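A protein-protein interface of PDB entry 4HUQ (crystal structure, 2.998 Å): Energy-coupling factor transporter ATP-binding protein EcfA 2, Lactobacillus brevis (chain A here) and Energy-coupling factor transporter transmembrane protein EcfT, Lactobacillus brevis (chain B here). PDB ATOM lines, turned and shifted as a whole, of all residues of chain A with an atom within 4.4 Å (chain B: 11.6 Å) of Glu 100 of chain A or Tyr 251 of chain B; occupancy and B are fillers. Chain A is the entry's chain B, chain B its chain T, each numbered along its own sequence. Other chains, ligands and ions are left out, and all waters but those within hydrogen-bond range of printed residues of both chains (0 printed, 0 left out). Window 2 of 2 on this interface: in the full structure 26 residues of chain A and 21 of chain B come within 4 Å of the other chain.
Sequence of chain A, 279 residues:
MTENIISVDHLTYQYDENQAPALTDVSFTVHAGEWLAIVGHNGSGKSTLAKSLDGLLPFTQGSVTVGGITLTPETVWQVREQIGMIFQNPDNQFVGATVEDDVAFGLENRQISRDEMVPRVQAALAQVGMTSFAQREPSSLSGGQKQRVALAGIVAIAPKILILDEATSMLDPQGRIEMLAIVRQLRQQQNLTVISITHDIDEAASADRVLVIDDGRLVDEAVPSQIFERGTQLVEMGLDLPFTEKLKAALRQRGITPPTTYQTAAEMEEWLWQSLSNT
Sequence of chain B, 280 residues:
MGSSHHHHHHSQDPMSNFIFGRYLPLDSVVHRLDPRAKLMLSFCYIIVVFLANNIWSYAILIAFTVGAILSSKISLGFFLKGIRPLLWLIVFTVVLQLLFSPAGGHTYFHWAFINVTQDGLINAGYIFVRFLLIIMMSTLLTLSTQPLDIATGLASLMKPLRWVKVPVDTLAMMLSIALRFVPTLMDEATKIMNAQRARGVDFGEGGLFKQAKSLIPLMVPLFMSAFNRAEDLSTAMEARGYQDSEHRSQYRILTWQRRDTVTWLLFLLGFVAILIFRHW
Of the 12 printed residues of chain A, 8 touch a printed residue of chain B. Hydrophobic or aromatic side chains of chain A within 4 Å of the printed part of chain B: Ala 104 and Met 117. Among the printed residues, Asp or Glu carboxylates within 4 Å of a Lys or Arg side-chain nitrogen of the other chain: Asp 101 of chain A with Arg 252 of chain B, Asp 102 of chain A with Arg 240 of chain B and Glu 108 of chain A with Arg 248 of chain B.
Among the printed residues, merely in contact across the chains: Glu 108 of chain A with Gln 250 of chain B (3.6 Å), Ala 104 of chain A with Tyr 251 of chain B (3.6 Å), Met 117 of chain A with Ser 249 of chain B (3.6 Å), Thr 98 of chain A with Arg 252 of chain B (3.9 Å) and Val 103 of chain A with Arg 240 of chain B (3.95 Å).
OG1 of Thr 98 of chain A sits at hydrogen-bond distance from O of Ala 134 of chain A (2.9 Å). The side-chain hydroxyl (OG1) of Thr 98 of chain A is in hydrogen-bond range of the backbone carbonyl oxygen (O) of Gln 135 of chain A, at 3.0 Å. The backbone carbonyl oxygen (O) of Ala 134 of chain A is in hydrogen-bond range of the backbone NH (N) of Glu 100 of chain A, at 3.2 Å. NH1 of Arg 252 of chain B lies within salt-bridge range of OD1 of Asp 149 of chain B (3.5 Å). The side-chain amino group (NZ) of Lys 159 of chain B lies close to the side-chain amide nitrogen (NE2) of Gln 250 of chain B. SD of Met 173 of chain B sits at hydrogen-bond distance from NH1 of Arg 248 of chain B (3.3 Å).
Of the printed residues of chain B, Glu 100 of chain A touches Tyr 251. Of the printed residues of chain A, Tyr 251 of chain B touches Glu 100 (3.3 Å), Ala 104 (3.6 Å) and Glu 108 (2.8 Å). Of the printed residues of chain B, Thr 98 of chain A touches Arg 252. Printed residues of chain B within 4 Å of Ala 104 of chain A: Tyr 251 (3.6 Å). Ala 134 of chain A touches none of the printed residues of chain B. Of the printed residues of chain A, Arg 240 of chain B touches Asp 102 and Val 103. Of the printed residues of chain A, Arg 248 of chain B touches Glu 108 (3.0 Å). Of the printed residues of chain B, Asp 101 of chain A touches Arg 252 (3.2 Å). The nearest printed residue of chain B that does not touch Glu 100 of chain A is Arg 252 of chain B (7.0 Å). The nearest printed residue of chain A that does not touch Tyr 251 of chain B is Asp 101 of chain A (4.01 Å). The nearest printed residue of chain B that does not touch Asp 101 of chain A is Tyr 251 of chain B (4.01 Å).
The side-chain hydroxyl (OH) of Tyr 251 of chain B sits close to the side-chain carboxylate (OE2) of Glu 100 of chain A (3.4 Å). The side-chain carboxylate (OD2) of Asp 101 of chain A is in salt-bridge range of the guanidinium group (NE) of Arg 252 of chain B. The side-chain carboxylate of Asp 102 of chain A lies within salt-bridge range of the guanidinium group of Arg 240 of chain B (3.6 Å). OE1 of Glu 108 of chain A is in salt-bridge range of NH2 of Arg 248 of chain B (3.7 Å). N of Ser 249 of chain B is in hydrogen-bond range of O of Glu 108 of chain A (3.1 Å). The backbone NH of Tyr 251 of chain B lies within hydrogen-bond range of the side-chain carboxylate of Glu 108 of chain A (2.8 Å).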
ATOM      1  N   THR A  98      -9.834  25.671  21.907  1.00  0.00           N
ATOM      2  CA  THR A  98     -10.385  26.659  22.827  1.00  0.00           C
ATOM      3  C   THR A  98     -10.719  27.978  22.119  1.00  0.00           C
ATOM      4  O   THR A  98     -10.444  28.147  20.929  1.00  0.00           O
ATOM      5  CB  THR A  98      -9.421  26.941  24.000  1.00  0.00           C
ATOM      6  OG1 THR A  98      -9.758  28.194  24.608  1.00  0.00           O
ATOM      7  CG2 THR A  98      -7.993  27.015  23.505  1.00  0.00           C
ATOM      8  N   VAL A  99     -11.308  28.907  22.869  1.00  0.00           N
ATOM      9  CA  VAL A  99     -11.749  30.186  22.320  1.00  0.00           C
ATOM     10  C   VAL A  99     -10.582  31.084  21.922  1.00  0.00           C
ATOM     11  O   VAL A  99     -10.540  31.594  20.796  1.00  0.00           O
ATOM     12  CB  VAL A  99     -12.672  30.931  23.306  1.00  0.00           C
ATOM     13  CG1 VAL A  99     -12.791  32.394  22.934  1.00  0.00           C
ATOM     14  CG2 VAL A  99     -14.028  30.302  23.306  1.00  0.00           C
ATOM     15  N   GLU A 100      -9.653  31.279  22.858  1.00  0.00           N
ATOM     16  CA  GLU A 100      -8.435  32.046  22.611  1.00  0.00           C
ATOM     17  C   GLU A 100      -7.827  31.630  21.286  1.00  0.00           C
ATOM     18  O   GLU A 100      -7.703  32.450  20.381  1.00  0.00           O
ATOM     19  CB  GLU A 100      -7.408  31.801  23.721  1.00  0.00           C
ATOM     20  CG  GLU A 100      -7.481  32.746  24.909  1.00  0.00           C
ATOM     21  CD  GLU A 100      -6.787  32.176  26.140  1.00  0.00           C
ATOM     22  OE1 GLU A 100      -6.832  30.933  26.313  1.00  0.00           O
ATOM     23  OE2 GLU A 100      -6.204  32.962  26.927  1.00  0.00           O
ATOM     24  N   ASP A 101      -7.465  30.349  21.192  1.00  0.00           N
ATOM     25  CA  ASP A 101      -6.861  29.769  19.993  1.00  0.00           C
ATOM     26  C   ASP A 101      -7.529  30.260  18.721  1.00  0.00           C
ATOM     27  O   ASP A 101      -6.857  30.731  17.797  1.00  0.00           O
ATOM     28  CB  ASP A 101      -6.944  28.241  20.042  1.00  0.00           C
ATOM     29  CG  ASP A 101      -5.830  27.626  20.847  1.00  0.00           C
ATOM     30  OD1 ASP A 101      -5.530  28.152  21.937  1.00  0.00           O
ATOM     31  OD2 ASP A 101      -5.250  26.622  20.385  1.00  0.00           O
ATOM     32  N   ASP A 102      -8.856  30.148  18.694  1.00  0.00           N
ATOM     33  CA  ASP A 102      -9.653  30.592  17.568  1.00  0.00           C
ATOM     34  C   ASP A 102      -9.449  32.085  17.274  1.00  0.00           C
ATOM     35  O   ASP A 102      -9.078  32.468  16.162  1.00  0.00           O
ATOM     36  CB  ASP A 102     -11.133  30.287  17.823  1.00  0.00           C
ATOM     37  CG  ASP A 102     -12.026  30.695  16.653  1.00  0.00           C
ATOM     38  OD1 ASP A 102     -11.602  30.520  15.491  1.00  0.00           O
ATOM     39  OD2 ASP A 102     -13.146  31.199  16.889  1.00  0.00           O
ATOM     40  N   VAL A 103      -9.684  32.921  18.279  1.00  0.00           N
ATOM     41  CA  VAL A 103      -9.630  34.363  18.108  1.00  0.00           C
ATOM     42  C   VAL A 103      -8.235  34.779  17.655  1.00  0.00           C
ATOM     43  O   VAL A 103      -8.051  35.840  17.048  1.00  0.00           O
ATOM     44  CB  VAL A 103     -10.048  35.074  19.414  1.00  0.00           C
ATOM     45  CG1 VAL A 103      -9.884  36.591  19.330  1.00  0.00           C
ATOM     46  CG2 VAL A 103     -11.481  34.724  19.739  1.00  0.00           C
ATOM     47  N   ALA A 104      -7.263  33.909  17.925  1.00  0.00           N
ATOM     48  CA  ALA A 104      -5.871  34.143  17.562  1.00  0.00           C
ATOM     49  C   ALA A 104      -5.482  33.498  16.228  1.00  0.00           C
ATOM     50  O   ALA A 104      -4.454  33.862  15.644  1.00  0.00           O
ATOM     51  CB  ALA A 104      -4.944  33.669  18.681  1.00  0.00           C
ATOM     52  N   GLU A 108      -2.535  34.675  13.767  1.00  0.00           N
ATOM     53  CA  GLU A 108      -1.441  33.757  13.467  1.00  0.00           C
ATOM     54  C   GLU A 108      -0.991  33.829  12.018  1.00  0.00           C
ATOM     55  O   GLU A 108       0.200  33.820  11.732  1.00  0.00           O
ATOM     56  CB  GLU A 108      -1.818  32.325  13.826  1.00  0.00           C
ATOM     57  CG  GLU A 108      -1.703  32.030  15.307  1.00  0.00           C
ATOM     58  CD  GLU A 108      -1.936  30.570  15.625  1.00  0.00           C
ATOM     59  OE1 GLU A 108      -2.712  29.917  14.879  1.00  0.00           O
ATOM     60  OE2 GLU A 108      -1.332  30.084  16.612  1.00  0.00           O
ATOM     61  N   MET A 117      -0.087  39.464  20.253  1.00  0.00           N
ATOM     62  CA  MET A 117      -1.314  38.679  20.187  1.00  0.00           C
ATOM     63  C   MET A 117      -2.080  38.644  21.503  1.00  0.00           C
ATOM     64  O   MET A 117      -3.303  38.746  21.508  1.00  0.00           O
ATOM     65  CB  MET A 117      -1.009  37.247  19.774  1.00  0.00           C
ATOM     66  CG  MET A 117      -0.665  37.063  18.322  1.00  0.00           C
ATOM     67  SD  MET A 117      -0.800  35.319  17.907  1.00  0.00           S
ATOM     68  CE  MET A 117      -0.143  35.316  16.261  1.00  0.00           C
ATOM     69  N   VAL A 121      -6.043  39.681  21.511  1.00  0.00           N
ATOM     70  CA  VAL A 121      -7.115  38.703  21.658  1.00  0.00           C
ATOM     71  C   VAL A 121      -7.887  38.943  22.959  1.00  0.00           C
ATOM     72  O   VAL A 121      -9.084  38.655  23.050  1.00  0.00           O
ATOM     73  CB  VAL A 121      -6.566  37.254  21.571  1.00  0.00           C
ATOM     74  CG1 VAL A 121      -7.593  36.233  22.045  1.00  0.00           C
ATOM     75  CG2 VAL A 121      -6.131  36.944  20.151  1.00  0.00           C
ATOM     76  N   ALA A 134     -13.071  32.605  27.625  1.00  0.00           N
ATOM     77  CA  ALA A 134     -11.838  32.481  26.834  1.00  0.00           C
ATOM     78  C   ALA A 134     -11.270  31.058  26.795  1.00  0.00           C
ATOM     79  O   ALA A 134     -10.569  30.682  25.848  1.00  0.00           O
ATOM     80  CB  ALA A 134     -10.785  33.466  27.301  1.00  0.00           C
ATOM     81  N   GLN A 135     -11.612  30.265  27.805  1.00  0.00           N
ATOM     82  CA  GLN A 135     -11.009  28.956  27.992  1.00  0.00           C
ATOM     83  C   GLN A 135     -11.756  27.833  27.278  1.00  0.00           C
ATOM     84  O   GLN A 135     -11.171  26.812  26.920  1.00  0.00           O
ATOM     85  CB  GLN A 135     -10.932  28.642  29.486  1.00  0.00           C
ATOM     86  CG  GLN A 135      -9.608  28.034  29.931  1.00  0.00           C
ATOM     87  CD  GLN A 135      -8.423  28.935  29.629  1.00  0.00           C
ATOM     88  OE1 GLN A 135      -8.355  30.075  30.093  1.00  0.00           O
ATOM     89  NE2 GLN A 135      -7.484  28.427  28.841  1.00  0.00           N
ATOM     90  N   GLN B 146      -3.483  16.136  29.255  1.00  0.00           N
ATOM     91  CA  GLN B 146      -4.586  16.486  28.374  1.00  0.00           C
ATOM     92  C   GLN B 146      -4.151  16.231  26.933  1.00  0.00           C
ATOM     93  O   GLN B 146      -3.023  16.562  26.556  1.00  0.00           O
ATOM     94  CB  GLN B 146      -4.981  17.949  28.580  1.00  0.00           C
ATOM     95  CG  GLN B 146      -5.149  18.326  30.044  1.00  0.00           C
ATOM     96  CD  GLN B 146      -5.907  19.625  30.239  1.00  0.00           C
ATOM     97  OE1 GLN B 146      -6.400  20.218  29.280  1.00  0.00           O
ATOM     98  NE2 GLN B 146      -6.010  20.071  31.488  1.00  0.00           N
ATOM     99  N   LEU B 148      -4.994  17.622  24.172  1.00  0.00           N
ATOM    100  CA  LEU B 148      -4.612  18.893  23.584  1.00  0.00           C
ATOM    101  C   LEU B 148      -3.164  19.225  23.955  1.00  0.00           C
ATOM    102  O   LEU B 148      -2.378  19.647  23.111  1.00  0.00           O
ATOM    103  CB  LEU B 148      -5.574  19.996  24.029  1.00  0.00           C
ATOM    104  CG  LEU B 148      -5.946  19.962  25.516  1.00  0.00           C
ATOM    105  CD1 LEU B 148      -6.137  21.381  26.049  1.00  0.00           C
ATOM    106  CD2 LEU B 148      -7.185  19.087  25.802  1.00  0.00           C
ATOM    107  N   ASP B 149      -2.800  19.006  25.213  1.00  0.00           N
ATOM    108  CA  ASP B 149      -1.425  19.249  25.630  1.00  0.00           C
ATOM    109  C   ASP B 149      -0.499  18.199  25.037  1.00  0.00           C
ATOM    110  O   ASP B 149       0.625  18.506  24.645  1.00  0.00           O
ATOM    111  CB  ASP B 149      -1.303  19.293  27.156  1.00  0.00           C
ATOM    112  CG  ASP B 149      -1.875  20.568  27.748  1.00  0.00           C
ATOM    113  OD1 ASP B 149      -2.179  21.508  26.970  1.00  0.00           O
ATOM    114  OD2 ASP B 149      -2.010  20.632  28.991  1.00  0.00           O
ATOM    115  N   THR B 152       0.023  19.391  21.562  1.00  0.00           N
ATOM    116  CA  THR B 152       0.922  20.539  21.557  1.00  0.00           C
ATOM    117  C   THR B 152       2.353  20.040  21.713  1.00  0.00           C
ATOM    118  O   THR B 152       3.295  20.631  21.166  1.00  0.00           O
ATOM    119  CB  THR B 152       0.634  21.522  22.717  1.00  0.00           C
ATOM    120  OG1 THR B 152      -0.770  21.784  22.828  1.00  0.00           O
ATOM    121  CG2 THR B 152       1.390  22.834  22.504  1.00  0.00           C
ATOM    122  N   ALA B 155       3.982  17.863  18.449  1.00  0.00           N
ATOM    123  CA  ALA B 155       4.381  18.840  17.440  1.00  0.00           C
ATOM    124  C   ALA B 155       5.792  19.363  17.686  1.00  0.00           C
ATOM    125  O   ALA B 155       6.553  19.567  16.741  1.00  0.00           O
ATOM    126  CB  ALA B 155       3.396  19.985  17.391  1.00  0.00           C
ATOM    127  N   SER B 156       6.146  19.574  18.950  1.00  0.00           N
ATOM    128  CA  SER B 156       7.525  19.922  19.285  1.00  0.00           C
ATOM    129  C   SER B 156       8.464  18.799  18.865  1.00  0.00           C
ATOM    130  O   SER B 156       9.326  18.985  18.012  1.00  0.00           O
ATOM    131  CB  SER B 156       7.684  20.207  20.783  1.00  0.00           C
ATOM    132  OG  SER B 156       7.254  21.518  21.113  1.00  0.00           O
ATOM    133  N   LYS B 159       9.219  18.429  15.220  1.00  0.00           N
ATOM    134  CA  LYS B 159       9.613  19.644  14.496  1.00  0.00           C
ATOM    135  C   LYS B 159      10.946  19.523  13.742  1.00  0.00           C
ATOM    136  O   LYS B 159      11.073  20.004  12.615  1.00  0.00           O
ATOM    137  CB  LYS B 159       9.607  20.857  15.442  1.00  0.00           C
ATOM    138  CG  LYS B 159       9.847  22.208  14.776  1.00  0.00           C
ATOM    139  CD  LYS B 159       9.327  23.361  15.656  1.00  0.00           C
ATOM    140  CE  LYS B 159       7.825  23.201  15.985  1.00  0.00           C
ATOM    141  NZ  LYS B 159       7.196  24.362  16.710  1.00  0.00           N
ATOM    142  N   ALA B 172       0.591  19.127  12.194  1.00  0.00           N
ATOM    143  CA  ALA B 172       0.153  19.725  13.451  1.00  0.00           C
ATOM    144  C   ALA B 172      -1.227  20.371  13.316  1.00  0.00           C
ATOM    145  O   ALA B 172      -2.016  20.364  14.256  1.00  0.00           O
ATOM    146  CB  ALA B 172       1.167  20.743  13.923  1.00  0.00           C
ATOM    147  N   MET B 173      -1.504  20.931  12.141  1.00  0.00           N
ATOM    148  CA  MET B 173      -2.818  21.491  11.840  1.00  0.00           C
ATOM    149  C   MET B 173      -3.883  20.405  11.632  1.00  0.00           C
ATOM    150  O   MET B 173      -4.966  20.472  12.213  1.00  0.00           O
ATOM    151  CB  MET B 173      -2.739  22.389  10.603  1.00  0.00           C
ATOM    152  CG  MET B 173      -4.013  23.182  10.308  1.00  0.00           C
ATOM    153  SD  MET B 173      -4.141  24.753  11.200  1.00  0.00           S
ATOM    154  CE  MET B 173      -4.898  24.275  12.756  1.00  0.00           C
ATOM    155  N   SER B 176      -4.822  19.027  14.883  1.00  0.00           N
ATOM    156  CA  SER B 176      -5.582  20.037  15.614  1.00  0.00           C
ATOM    157  C   SER B 176      -7.046  20.055  15.174  1.00  0.00           C
ATOM    158  O   SER B 176      -7.961  20.027  16.007  1.00  0.00           O
ATOM    159  CB  SER B 176      -4.963  21.416  15.418  1.00  0.00           C
ATOM    160  OG  SER B 176      -4.455  21.902  16.645  1.00  0.00           O
ATOM    161  N   ARG B 240     -10.798  33.822   6.802  1.00  0.00           N
ATOM    162  CA  ARG B 240      -9.756  34.275   7.695  1.00  0.00           C
ATOM    163  C   ARG B 240      -8.518  34.043   6.860  1.00  0.00           C
ATOM    164  O   ARG B 240      -8.517  33.155   6.012  1.00  0.00           O
ATOM    165  CB  ARG B 240      -9.716  33.425   8.960  1.00  0.00           C
ATOM    166  CG  ARG B 240     -10.155  34.158  10.215  1.00  0.00           C
ATOM    167  CD  ARG B 240     -11.402  33.529  10.811  1.00  0.00           C
ATOM    168  NE  ARG B 240     -11.585  33.902  12.210  1.00  0.00           N
ATOM    169  CZ  ARG B 240     -10.788  33.510  13.197  1.00  0.00           C
ATOM    170  NH1 ARG B 240      -9.749  32.730  12.940  1.00  0.00           N
ATOM    171  NH2 ARG B 240     -11.030  33.896  14.442  1.00  0.00           N
ATOM    172  N   SER B 245       0.517  26.085   5.787  1.00  0.00           N
ATOM    173  CA  SER B 245       0.704  25.651   7.165  1.00  0.00           C
ATOM    174  C   SER B 245       1.853  26.430   7.784  1.00  0.00           C
ATOM    175  O   SER B 245       1.811  26.815   8.951  1.00  0.00           O
ATOM    176  CB  SER B 245       1.002  24.152   7.214  1.00  0.00           C
ATOM    177  OG  SER B 245       1.044  23.679   8.548  1.00  0.00           O
ATOM    178  N   HIS B 247       4.911  29.577   7.586  1.00  0.00           N
ATOM    179  CA  HIS B 247       4.839  31.028   7.458  1.00  0.00           C
ATOM    180  C   HIS B 247       3.769  31.660   8.353  1.00  0.00           C
ATOM    181  O   HIS B 247       3.158  32.663   7.983  1.00  0.00           O
ATOM    182  CB  HIS B 247       4.642  31.430   5.985  1.00  0.00           C
ATOM    183  CG  HIS B 247       5.754  30.985   5.082  1.00  0.00           C
ATOM    184  ND1 HIS B 247       6.984  31.611   5.051  1.00  0.00           N
ATOM    185  CD2 HIS B 247       5.823  29.977   4.181  1.00  0.00           C
ATOM    186  CE1 HIS B 247       7.761  31.007   4.169  1.00  0.00           C
ATOM    187  NE2 HIS B 247       7.082  30.011   3.629  1.00  0.00           N
ATOM    188  N   ARG B 248       3.540  31.056   9.517  1.00  0.00           N
ATOM    189  CA  ARG B 248       2.669  31.644  10.535  1.00  0.00           C
ATOM    190  C   ARG B 248       3.119  31.340  11.965  1.00  0.00           C
ATOM    191  O   ARG B 248       4.068  30.586  12.187  1.00  0.00           O
ATOM    192  CB  ARG B 248       1.178  31.296  10.334  1.00  0.00           C
ATOM    193  CG  ARG B 248       0.829  29.887   9.877  1.00  0.00           C
ATOM    194  CD  ARG B 248      -0.551  29.455  10.404  1.00  0.00           C
ATOM    195  NE  ARG B 248      -0.420  28.764  11.683  1.00  0.00           N
ATOM    196  CZ  ARG B 248      -1.159  27.734  12.068  1.00  0.00           C
ATOM    197  NH1 ARG B 248      -2.110  27.290  11.271  1.00  0.00           N
ATOM    198  NH2 ARG B 248      -0.939  27.157  13.249  1.00  0.00           N
ATOM    199  N   SER B 249       2.404  31.922  12.924  1.00  0.00           N
ATOM    200  CA  SER B 249       2.848  31.915  14.313  1.00  0.00           C
ATOM    201  C   SER B 249       2.259  30.801  15.170  1.00  0.00           C
ATOM    202  O   SER B 249       1.464  29.970  14.715  1.00  0.00           O
ATOM    203  CB  SER B 249       2.507  33.247  14.975  1.00  0.00           C
ATOM    204  OG  SER B 249       3.675  33.909  15.418  1.00  0.00           O
ATOM    205  N   GLN B 250       2.686  30.810  16.433  1.00  0.00           N
ATOM    206  CA  GLN B 250       2.146  29.903  17.421  1.00  0.00           C
ATOM    207  C   GLN B 250       1.649  30.692  18.615  1.00  0.00           C
ATOM    208  O   GLN B 250       2.444  31.255  19.369  1.00  0.00           O
ATOM    209  CB  GLN B 250       3.196  28.880  17.854  1.00  0.00           C
ATOM    210  CG  GLN B 250       3.219  27.622  16.998  1.00  0.00           C
ATOM    211  CD  GLN B 250       4.129  26.536  17.564  1.00  0.00           C
ATOM    212  OE1 GLN B 250       4.860  26.755  18.537  1.00  0.00           O
ATOM    213  NE2 GLN B 250       4.086  25.354  16.953  1.00  0.00           N
ATOM    214  N   TYR B 251       0.330  30.757  18.764  1.00  0.00           N
ATOM    215  CA  TYR B 251      -0.272  31.356  19.944  1.00  0.00           C
ATOM    216  C   TYR B 251      -0.166  30.380  21.124  1.00  0.00           C
ATOM    217  O   TYR B 251      -0.052  30.792  22.285  1.00  0.00           O
ATOM    218  CB  TYR B 251      -1.735  31.723  19.661  1.00  0.00           C
ATOM    219  CG  TYR B 251      -2.464  32.287  20.863  1.00  0.00           C
ATOM    220  CD1 TYR B 251      -2.147  33.547  21.361  1.00  0.00           C
ATOM    221  CD2 TYR B 251      -3.458  31.559  21.509  1.00  0.00           C
ATOM    222  CE1 TYR B 251      -2.806  34.072  22.465  1.00  0.00           C
ATOM    223  CE2 TYR B 251      -4.117  32.073  22.617  1.00  0.00           C
ATOM    224  CZ  TYR B 251      -3.792  33.333  23.089  1.00  0.00           C
ATOM    225  OH  TYR B 251      -4.441  33.865  24.184  1.00  0.00           O
ATOM    226  N   ARG B 252      -0.213  29.083  20.815  1.00  0.00           N
ATOM    227  CA  ARG B 252      -0.074  28.042  21.828  1.00  0.00           C
ATOM    228  C   ARG B 252       1.394  27.795  22.102  1.00  0.00           C
ATOM    229  O   ARG B 252       2.153  27.373  21.225  1.00  0.00           O
ATOM    230  CB  ARG B 252      -0.762  26.747  21.402  1.00  0.00           C
ATOM    231  CG  ARG B 252      -1.799  26.283  22.409  1.00  0.00           C
ATOM    232  CD  ARG B 252      -2.512  25.012  21.988  1.00  0.00           C
ATOM    233  NE  ARG B 252      -3.818  24.947  22.638  1.00  0.00           N
ATOM    234  CZ  ARG B 252      -4.028  24.440  23.849  1.00  0.00           C
ATOM    235  NH1 ARG B 252      -3.018  23.926  24.549  1.00  0.00           N
ATOM    236  NH2 ARG B 252      -5.250  24.443  24.363  1.00  0.00           N
ATOM    237  N   ILE B 253       1.789  28.069  23.335  1.00  0.00           N
ATOM    238  CA  ILE B 253       3.193  28.137  23.685  1.00  0.00           C
ATOM    239  C   ILE B 253       3.474  27.104  24.785  1.00  0.00           C
ATOM    240  O   ILE B 253       2.655  26.916  25.688  1.00  0.00           O
ATOM    241  CB  ILE B 253       3.568  29.593  24.123  1.00  0.00           C
ATOM    242  CG1 ILE B 253       2.919  30.642  23.180  1.00  0.00           C
ATOM    243  CG2 ILE B 253       5.056  29.770  24.133  1.00  0.00           C
ATOM    244  CD1 ILE B 253       2.453  32.021  23.824  1.00  0.00           C
ATOM    245  N   LEU B 254       4.605  26.406  24.683  1.00  0.00           N
ATOM    246  CA  LEU B 254       5.014  25.447  25.709  1.00  0.00           C
ATOM    247  C   LEU B 254       6.181  25.995  26.514  1.00  0.00           C
ATOM    248  O   LEU B 254       7.202  26.383  25.948  1.00  0.00           O
ATOM    249  CB  LEU B 254       5.402  24.107  25.086  1.00  0.00           C
ATOM    250  CG  LEU B 254       4.269  23.149  24.698  1.00  0.00           C
ATOM    251  CD1 LEU B 254       4.821  21.986  23.882  1.00  0.00           C
ATOM    252  CD2 LEU B 254       3.489  22.631  25.916  1.00  0.00           C
ATOM    253  N   THR B 255       6.035  26.026  27.834  1.00  0.00           N
ATOM    254  CA  THR B 255       7.089  26.548  28.698  1.00  0.00           C
ATOM    255  C   THR B 255       7.781  25.424  29.462  1.00  0.00           C
ATOM    256  O   THR B 255       7.175  24.800  30.328  1.00  0.00           O
ATOM    257  CB  THR B 255       6.533  27.569  29.724  1.00  0.00           C
ATOM    258  OG1 THR B 255       5.845  26.880  30.778  1.00  0.00           O
ATOM    259  CG2 THR B 255       5.575  28.541  29.055  1.00  0.00           C
